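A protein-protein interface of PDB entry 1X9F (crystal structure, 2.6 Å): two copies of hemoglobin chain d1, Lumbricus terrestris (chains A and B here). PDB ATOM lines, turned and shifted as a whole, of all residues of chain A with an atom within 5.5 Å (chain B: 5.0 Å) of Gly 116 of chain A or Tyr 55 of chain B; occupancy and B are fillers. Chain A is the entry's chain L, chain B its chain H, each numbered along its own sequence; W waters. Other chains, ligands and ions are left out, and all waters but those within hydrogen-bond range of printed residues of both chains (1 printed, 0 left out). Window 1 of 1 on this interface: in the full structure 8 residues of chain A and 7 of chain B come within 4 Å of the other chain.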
ATOM      1  N   LEU A 111     -15.844 -24.342 -27.482  1.00  0.00           N
ATOM      2  CA  LEU A 111     -15.897 -22.883 -27.494  1.00  0.00           C
ATOM      3  C   LEU A 111     -15.734 -22.345 -26.078  1.00  0.00           C
ATOM      4  O   LEU A 111     -14.942 -21.434 -25.851  1.00  0.00           O
ATOM      5  CB  LEU A 111     -17.199 -22.370 -28.124  1.00  0.00           C
ATOM      6  CG  LEU A 111     -17.438 -20.854 -28.171  1.00  0.00           C
ATOM      7  CD1 LEU A 111     -16.385 -20.137 -29.017  1.00  0.00           C
ATOM      8  CD2 LEU A 111     -18.829 -20.560 -28.695  1.00  0.00           C
ATOM      9  N   LEU A 112     -16.468 -22.920 -25.131  1.00  0.00           N
ATOM     10  CA  LEU A 112     -16.404 -22.457 -23.749  1.00  0.00           C
ATOM     11  C   LEU A 112     -15.044 -22.747 -23.109  1.00  0.00           C
ATOM     12  O   LEU A 112     -14.568 -21.970 -22.274  1.00  0.00           O
ATOM     13  CB  LEU A 112     -17.552 -23.038 -22.916  1.00  0.00           C
ATOM     14  CG  LEU A 112     -18.990 -22.717 -23.346  1.00  0.00           C
ATOM     15  CD1 LEU A 112     -19.961 -23.134 -22.257  1.00  0.00           C
ATOM     16  CD2 LEU A 112     -19.178 -21.237 -23.669  1.00  0.00           C
ATOM     17  N   HIS A 113     -14.426 -23.856 -23.518  1.00  0.00           N
ATOM     18  CA  HIS A 113     -13.085 -24.225 -23.068  1.00  0.00           C
ATOM     19  C   HIS A 113     -12.034 -23.213 -23.548  1.00  0.00           C
ATOM     20  O   HIS A 113     -11.269 -22.673 -22.739  1.00  0.00           O
ATOM     21  CB  HIS A 113     -12.740 -25.651 -23.522  1.00  0.00           C
ATOM     22  CG  HIS A 113     -11.504 -26.212 -22.885  1.00  0.00           C
ATOM     23  ND1 HIS A 113     -10.235 -25.890 -23.316  1.00  0.00           N
ATOM     24  CD2 HIS A 113     -11.342 -27.082 -21.859  1.00  0.00           C
ATOM     25  CE1 HIS A 113      -9.345 -26.528 -22.578  1.00  0.00           C
ATOM     26  NE2 HIS A 113      -9.991 -27.257 -21.685  1.00  0.00           N
ATOM     27  N   VAL A 114     -11.996 -22.939 -24.850  1.00  0.00           N
ATOM     28  CA  VAL A 114     -11.024 -21.976 -25.370  1.00  0.00           C
ATOM     29  C   VAL A 114     -11.299 -20.580 -24.835  1.00  0.00           C
ATOM     30  O   VAL A 114     -10.363 -19.821 -24.567  1.00  0.00           O
ATOM     31  CB  VAL A 114     -10.931 -21.956 -26.922  1.00  0.00           C
ATOM     32  CG1 VAL A 114     -10.502 -23.325 -27.455  1.00  0.00           C
ATOM     33  CG2 VAL A 114     -12.241 -21.530 -27.563  1.00  0.00           C
ATOM     34  N   LEU A 115     -12.579 -20.245 -24.679  1.00  0.00           N
ATOM     35  CA  LEU A 115     -12.956 -18.947 -24.133  1.00  0.00           C
ATOM     36  C   LEU A 115     -12.461 -18.802 -22.700  1.00  0.00           C
ATOM     37  O   LEU A 115     -12.021 -17.726 -22.296  1.00  0.00           O
ATOM     38  CB  LEU A 115     -14.469 -18.726 -24.200  1.00  0.00           C
ATOM     39  CG  LEU A 115     -15.083 -18.301 -25.539  1.00  0.00           C
ATOM     40  CD1 LEU A 115     -16.589 -18.460 -25.491  1.00  0.00           C
ATOM     41  CD2 LEU A 115     -14.702 -16.876 -25.911  1.00  0.00           C
ATOM     42  N   GLY A 116     -12.529 -19.896 -21.945  1.00  0.00           N
ATOM     43  CA  GLY A 116     -12.055 -19.930 -20.566  1.00  0.00           C
ATOM     44  C   GLY A 116     -10.570 -19.640 -20.473  1.00  0.00           C
ATOM     45  O   GLY A 116     -10.125 -18.958 -19.545  1.00  0.00           O
ATOM     46  N   ASP A 117      -9.810 -20.158 -21.439  1.00  0.00           N
ATOM     47  CA  ASP A 117      -8.366 -19.906 -21.536  1.00  0.00           C
ATOM     48  C   ASP A 117      -8.068 -18.443 -21.781  1.00  0.00           C
ATOM     49  O   ASP A 117      -7.191 -17.871 -21.138  1.00  0.00           O
ATOM     50  CB  ASP A 117      -7.734 -20.725 -22.668  1.00  0.00           C
ATOM     51  CG  ASP A 117      -7.620 -22.199 -22.334  1.00  0.00           C
ATOM     52  OD1 ASP A 117      -7.400 -22.538 -21.153  1.00  0.00           O
ATOM     53  OD2 ASP A 117      -7.724 -23.097 -23.197  1.00  0.00           O
ATOM     54  N   ARG A 118      -8.797 -17.856 -22.724  1.00  0.00           N
ATOM     55  CA  ARG A 118      -8.600 -16.477 -23.131  1.00  0.00           C
ATOM     56  C   ARG A 118      -8.988 -15.491 -22.044  1.00  0.00           C
ATOM     57  O   ARG A 118      -8.300 -14.494 -21.836  1.00  0.00           O
ATOM     58  CB  ARG A 118      -9.435 -16.188 -24.374  1.00  0.00           C
ATOM     59  CG  ARG A 118      -8.873 -16.769 -25.645  1.00  0.00           C
ATOM     60  CD  ARG A 118      -7.633 -16.038 -26.130  1.00  0.00           C
ATOM     61  NE  ARG A 118      -7.095 -16.565 -27.382  1.00  0.00           N
ATOM     62  CZ  ARG A 118      -6.923 -17.852 -27.670  1.00  0.00           C
ATOM     63  NH1 ARG A 118      -7.228 -18.802 -26.792  1.00  0.00           N
ATOM     64  NH2 ARG A 118      -6.424 -18.194 -28.849  1.00  0.00           N
ATOM     65  N   LEU A 119     -10.094 -15.768 -21.357  1.00  0.00           N
ATOM     66  CA  LEU A 119     -10.692 -14.806 -20.426  1.00  0.00           C
ATOM     67  C   LEU A 119     -10.299 -15.038 -18.970  1.00  0.00           C
ATOM     68  O   LEU A 119     -10.329 -14.112 -18.158  1.00  0.00           O
ATOM     69  CB  LEU A 119     -12.219 -14.795 -20.564  1.00  0.00           C
ATOM     70  CG  LEU A 119     -12.819 -14.256 -21.866  1.00  0.00           C
ATOM     71  CD1 LEU A 119     -14.283 -14.648 -21.970  1.00  0.00           C
ATOM     72  CD2 LEU A 119     -12.662 -12.742 -21.975  1.00  0.00           C
ATOM     73  N   GLY A 120      -9.944 -16.278 -18.647  1.00  0.00           N
ATOM     74  CA  GLY A 120      -9.494 -16.625 -17.305  1.00  0.00           C
ATOM     75  C   GLY A 120     -10.634 -16.844 -16.334  1.00  0.00           C
ATOM     76  O   GLY A 120     -11.743 -17.207 -16.728  1.00  0.00           O
ATOM     77  N   THR A 121     -10.356 -16.609 -15.059  1.00  0.00           N
ATOM     78  CA  THR A 121     -11.314 -16.879 -13.995  1.00  0.00           C
ATOM     79  C   THR A 121     -12.520 -15.938 -14.056  1.00  0.00           C
ATOM     80  O   THR A 121     -13.486 -16.109 -13.315  1.00  0.00           O
ATOM     81  CB  THR A 121     -10.623 -16.775 -12.622  1.00  0.00           C
ATOM     82  OG1 THR A 121     -10.774 -15.436 -12.115  1.00  0.00           O
ATOM     83  CG2 THR A 121      -9.091 -16.931 -12.775  1.00  0.00           C
ATOM     84  N   HIS A 122     -12.454 -14.951 -14.946  1.00  0.00           N
ATOM     85  CA  HIS A 122     -13.517 -13.966 -15.126  1.00  0.00           C
ATOM     86  C   HIS A 122     -14.614 -14.449 -16.061  1.00  0.00           C
ATOM     87  O   HIS A 122     -15.710 -13.880 -16.096  1.00  0.00           O
ATOM     88  CB  HIS A 122     -12.938 -12.664 -15.682  1.00  0.00           C
ATOM     89  CG  HIS A 122     -12.129 -11.890 -14.690  1.00  0.00           C
ATOM     90  ND1 HIS A 122     -12.422 -11.875 -13.343  1.00  0.00           N
ATOM     91  CD2 HIS A 122     -11.050 -11.087 -14.849  1.00  0.00           C
ATOM     92  CE1 HIS A 122     -11.552 -11.106 -12.713  1.00  0.00           C
ATOM     93  NE2 HIS A 122     -10.711 -10.612 -13.604  1.00  0.00           N
ATOM     94  N   PHE A 123     -14.302 -15.481 -16.832  1.00  0.00           N
ATOM     95  CA  PHE A 123     -15.223 -16.061 -17.795  1.00  0.00           C
ATOM     96  C   PHE A 123     -16.595 -16.323 -17.165  1.00  0.00           C
ATOM     97  O   PHE A 123     -16.715 -17.131 -16.242  1.00  0.00           O
ATOM     98  CB  PHE A 123     -14.591 -17.345 -18.328  1.00  0.00           C
ATOM     99  CG  PHE A 123     -15.426 -18.092 -19.316  1.00  0.00           C
ATOM    100  CD1 PHE A 123     -15.966 -17.459 -20.433  1.00  0.00           C
ATOM    101  CD2 PHE A 123     -15.624 -19.460 -19.154  1.00  0.00           C
ATOM    102  CE1 PHE A 123     -16.719 -18.175 -21.354  1.00  0.00           C
ATOM    103  CE2 PHE A 123     -16.372 -20.185 -20.065  1.00  0.00           C
ATOM    104  CZ  PHE A 123     -16.924 -19.541 -21.171  1.00  0.00           C
ATOM    105  N   PHE A 125     -19.091 -18.199 -17.424  1.00  0.00           N
ATOM    106  CA  PHE A 125     -19.527 -19.509 -17.886  1.00  0.00           C
ATOM    107  C   PHE A 125     -21.035 -19.660 -17.910  1.00  0.00           C
ATOM    108  O   PHE A 125     -21.597 -20.147 -18.891  1.00  0.00           O
ATOM    109  CB  PHE A 125     -18.947 -20.580 -16.964  1.00  0.00           C
ATOM    110  CG  PHE A 125     -19.257 -21.984 -17.392  1.00  0.00           C
ATOM    111  CD1 PHE A 125     -20.324 -22.682 -16.832  1.00  0.00           C
ATOM    112  CD2 PHE A 125     -18.473 -22.614 -18.350  1.00  0.00           C
ATOM    113  CE1 PHE A 125     -20.608 -23.988 -17.229  1.00  0.00           C
ATOM    114  CE2 PHE A 125     -18.748 -23.921 -18.754  1.00  0.00           C
ATOM    115  CZ  PHE A 125     -19.816 -24.608 -18.191  1.00  0.00           C
ATOM    116  N   LEU B  29      -8.764 -23.460 -10.555  1.00  0.00           N
ATOM    117  CA  LEU B  29      -9.755 -23.568 -11.607  1.00  0.00           C
ATOM    118  C   LEU B  29      -9.212 -24.444 -12.739  1.00  0.00           C
ATOM    119  O   LEU B  29      -9.873 -25.403 -13.157  1.00  0.00           O
ATOM    120  CB  LEU B  29     -10.122 -22.172 -12.107  1.00  0.00           C
ATOM    121  CG  LEU B  29     -10.878 -22.076 -13.434  1.00  0.00           C
ATOM    122  CD1 LEU B  29     -12.368 -22.003 -13.183  1.00  0.00           C
ATOM    123  CD2 LEU B  29     -10.408 -20.859 -14.222  1.00  0.00           C
ATOM    124  N   ARG B  33     -11.032 -27.951 -13.770  1.00  0.00           N
ATOM    125  CA  ARG B  33     -11.538 -28.022 -15.130  1.00  0.00           C
ATOM    126  C   ARG B  33     -10.988 -29.247 -15.846  1.00  0.00           C
ATOM    127  O   ARG B  33     -11.750 -29.991 -16.462  1.00  0.00           O
ATOM    128  CB  ARG B  33     -11.245 -26.773 -15.944  1.00  0.00           C
ATOM    129  CG  ARG B  33     -11.992 -26.844 -17.263  1.00  0.00           C
ATOM    130  CD  ARG B  33     -11.808 -25.676 -18.161  1.00  0.00           C
ATOM    131  NE  ARG B  33     -10.429 -25.526 -18.601  1.00  0.00           N
ATOM    132  CZ  ARG B  33     -10.026 -24.564 -19.414  1.00  0.00           C
ATOM    133  NH1 ARG B  33     -10.893 -23.673 -19.878  1.00  0.00           N
ATOM    134  NH2 ARG B  33      -8.752 -24.487 -19.771  1.00  0.00           N
ATOM    135  N   ASN B  53     -20.717 -25.225 -12.547  1.00  0.00           N
ATOM    136  CA  ASN B  53     -20.131 -23.976 -13.011  1.00  0.00           C
ATOM    137  C   ASN B  53     -18.885 -23.655 -12.184  1.00  0.00           C
ATOM    138  O   ASN B  53     -18.973 -23.022 -11.129  1.00  0.00           O
ATOM    139  CB  ASN B  53     -21.159 -22.844 -12.917  1.00  0.00           C
ATOM    140  CG  ASN B  53     -20.608 -21.513 -13.385  1.00  0.00           C
ATOM    141  OD1 ASN B  53     -19.479 -21.421 -13.870  1.00  0.00           O
ATOM    142  ND2 ASN B  53     -21.408 -20.466 -13.239  1.00  0.00           N
ATOM    143  N   ILE B  54     -17.729 -24.095 -12.670  1.00  0.00           N
ATOM    144  CA  ILE B  54     -16.474 -23.960 -11.923  1.00  0.00           C
ATOM    145  C   ILE B  54     -15.958 -22.523 -11.868  1.00  0.00           C
ATOM    146  O   ILE B  54     -14.998 -22.225 -11.151  1.00  0.00           O
ATOM    147  CB  ILE B  54     -15.392 -24.888 -12.503  1.00  0.00           C
ATOM    148  CG1 ILE B  54     -15.164 -24.578 -13.988  1.00  0.00           C
ATOM    149  CG2 ILE B  54     -15.778 -26.348 -12.284  1.00  0.00           C
ATOM    150  CD1 ILE B  54     -13.849 -25.058 -14.528  1.00  0.00           C
ATOM    151  N   TYR B  55     -16.598 -21.647 -12.634  1.00  0.00           N
ATOM    152  CA  TYR B  55     -16.216 -20.248 -12.705  1.00  0.00           C
ATOM    153  C   TYR B  55     -17.082 -19.415 -11.781  1.00  0.00           C
ATOM    154  O   TYR B  55     -16.943 -18.192 -11.721  1.00  0.00           O
ATOM    155  CB  TYR B  55     -16.355 -19.729 -14.134  1.00  0.00           C
ATOM    156  CG  TYR B  55     -15.447 -20.400 -15.136  1.00  0.00           C
ATOM    157  CD1 TYR B  55     -15.820 -21.590 -15.755  1.00  0.00           C
ATOM    158  CD2 TYR B  55     -14.220 -19.836 -15.474  1.00  0.00           C
ATOM    159  CE1 TYR B  55     -14.992 -22.205 -16.679  1.00  0.00           C
ATOM    160  CE2 TYR B  55     -13.385 -20.444 -16.396  1.00  0.00           C
ATOM    161  CZ  TYR B  55     -13.775 -21.626 -16.994  1.00  0.00           C
ATOM    162  OH  TYR B  55     -12.944 -22.227 -17.909  1.00  0.00           O
ATOM    163  N   SER B  56     -17.986 -20.072 -11.061  1.00  0.00           N
ATOM    164  CA  SER B  56     -18.831 -19.361 -10.111  1.00  0.00           C
ATOM    165  C   SER B  56     -18.030 -19.066  -8.845  1.00  0.00           C
ATOM    166  O   SER B  56     -17.035 -19.752  -8.565  1.00  0.00           O
ATOM    167  CB  SER B  56     -20.068 -20.190  -9.777  1.00  0.00           C
ATOM    168  OG  SER B  56     -19.709 -21.356  -9.058  1.00  0.00           O
ATOM    169  N   PRO B  57     -18.444 -18.063  -8.070  1.00  0.00           N
ATOM    170  CA  PRO B  57     -17.718 -17.736  -6.853  1.00  0.00           C
ATOM    171  C   PRO B  57     -17.824 -18.848  -5.800  1.00  0.00           C
ATOM    172  O   PRO B  57     -16.912 -18.991  -4.983  1.00  0.00           O
ATOM    173  CB  PRO B  57     -18.389 -16.444  -6.372  1.00  0.00           C
ATOM    174  CG  PRO B  57     -19.751 -16.465  -6.968  1.00  0.00           C
ATOM    175  CD  PRO B  57     -19.615 -17.184  -8.272  1.00  0.00           C
HETATM  176  O   HOH W   1     -14.053 -23.710 -19.726  1.00  0.00           O
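The guanidinium group (NH2) of Arg 33 of chain B is in salt-bridge range of the side-chain carboxylate (OD1) of Asp 117 of chain A (2.7 Å). The guanidinium group of Arg 33 of chain B is in hydrogen-bond range of the backbone carbonyl oxygen of His 113 of chain A, 3.1 Å away.
OH of Tyr 55 of chain B is in hydrogen-bond range of NH1 of Arg 33 of chain B (3.2 Å). N of Tyr 55 of chain B sits close to OD1 of Asn 53 of chain B (3.1 Å). O of Asn 53 of chain B lies within hydrogen-bond range of OG of Ser 56 of chain B (2.8 Å).
Among the printed residues, pairs that only touch across the chains: Phe 125 of chain A with Asn 53 of chain B (3.3 Å), Phe 123 of chain A with Tyr 55 of chain B (3.4 Å), Phe 125 of chain A with Tyr 55 of chain B (3.5 Å), Gly 116 of chain A with Tyr 55 of chain B (3.6 Å), Gly 120 of chain A with Tyr 55 of chain B (3.6 Å) and Gly 116 of chain A with Arg 33 of chain B (3.98 Å).
Leu 111 of chain A touches none of the printed residues of chain B. Gly 116 of chain A touches two residues of chain B. Printed residues of chain B within 4 Å of Asp 117 of chain A: Arg 33. Of the printed residues of chain B, Gly 120 of chain A touches Tyr 55 (3.6 Å). Of the printed residues of chain B, Phe 123 of chain A touches Tyr 55. Printed residues of chain B within 4 Å of Phe 125 of chain A: Asn 53 and Tyr 55. Of the printed residues of chain A, Asn 53 of chain B touches Phe 125. Tyr 55 of chain B touches just these residues of chain A: Gly 116, Gly 120, Phe 123 and Phe 125. Ser 56 of chain B touches none of the printed residues of chain A. The nearest printed residue of chain B that does not touch Phe 123 of chain A is Asn 53 of chain B (5.6 Å).
Of the 14 printed residues of chain A, 6 touch a printed residue of chain B. Hydrophobic or aromatic side chains of chain A within 4 Å of the printed part of chain B: His 113, Phe 123 and Phe 125. Hydrophobic or aromatic side chains of chain B that line the printed part of chain A: Tyr 55. Among the printed residues, 8 pairs touch across the chains. Among the printed residues, Asp or Glu carboxylates within 4 Å of a Lys or Arg side-chain nitrogen of the other chain: Asp 117 of chain A with Arg 33 of chain B (2.7 Å).
No position is printed for both chains.
Water W1 lies within hydrogen-bond range of OH of Tyr 55 of chain B (2.6 Å), O of Leu 112 of chain A (3.1 Å) and NH1 of Arg 33 of chain B (3.2 Å).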
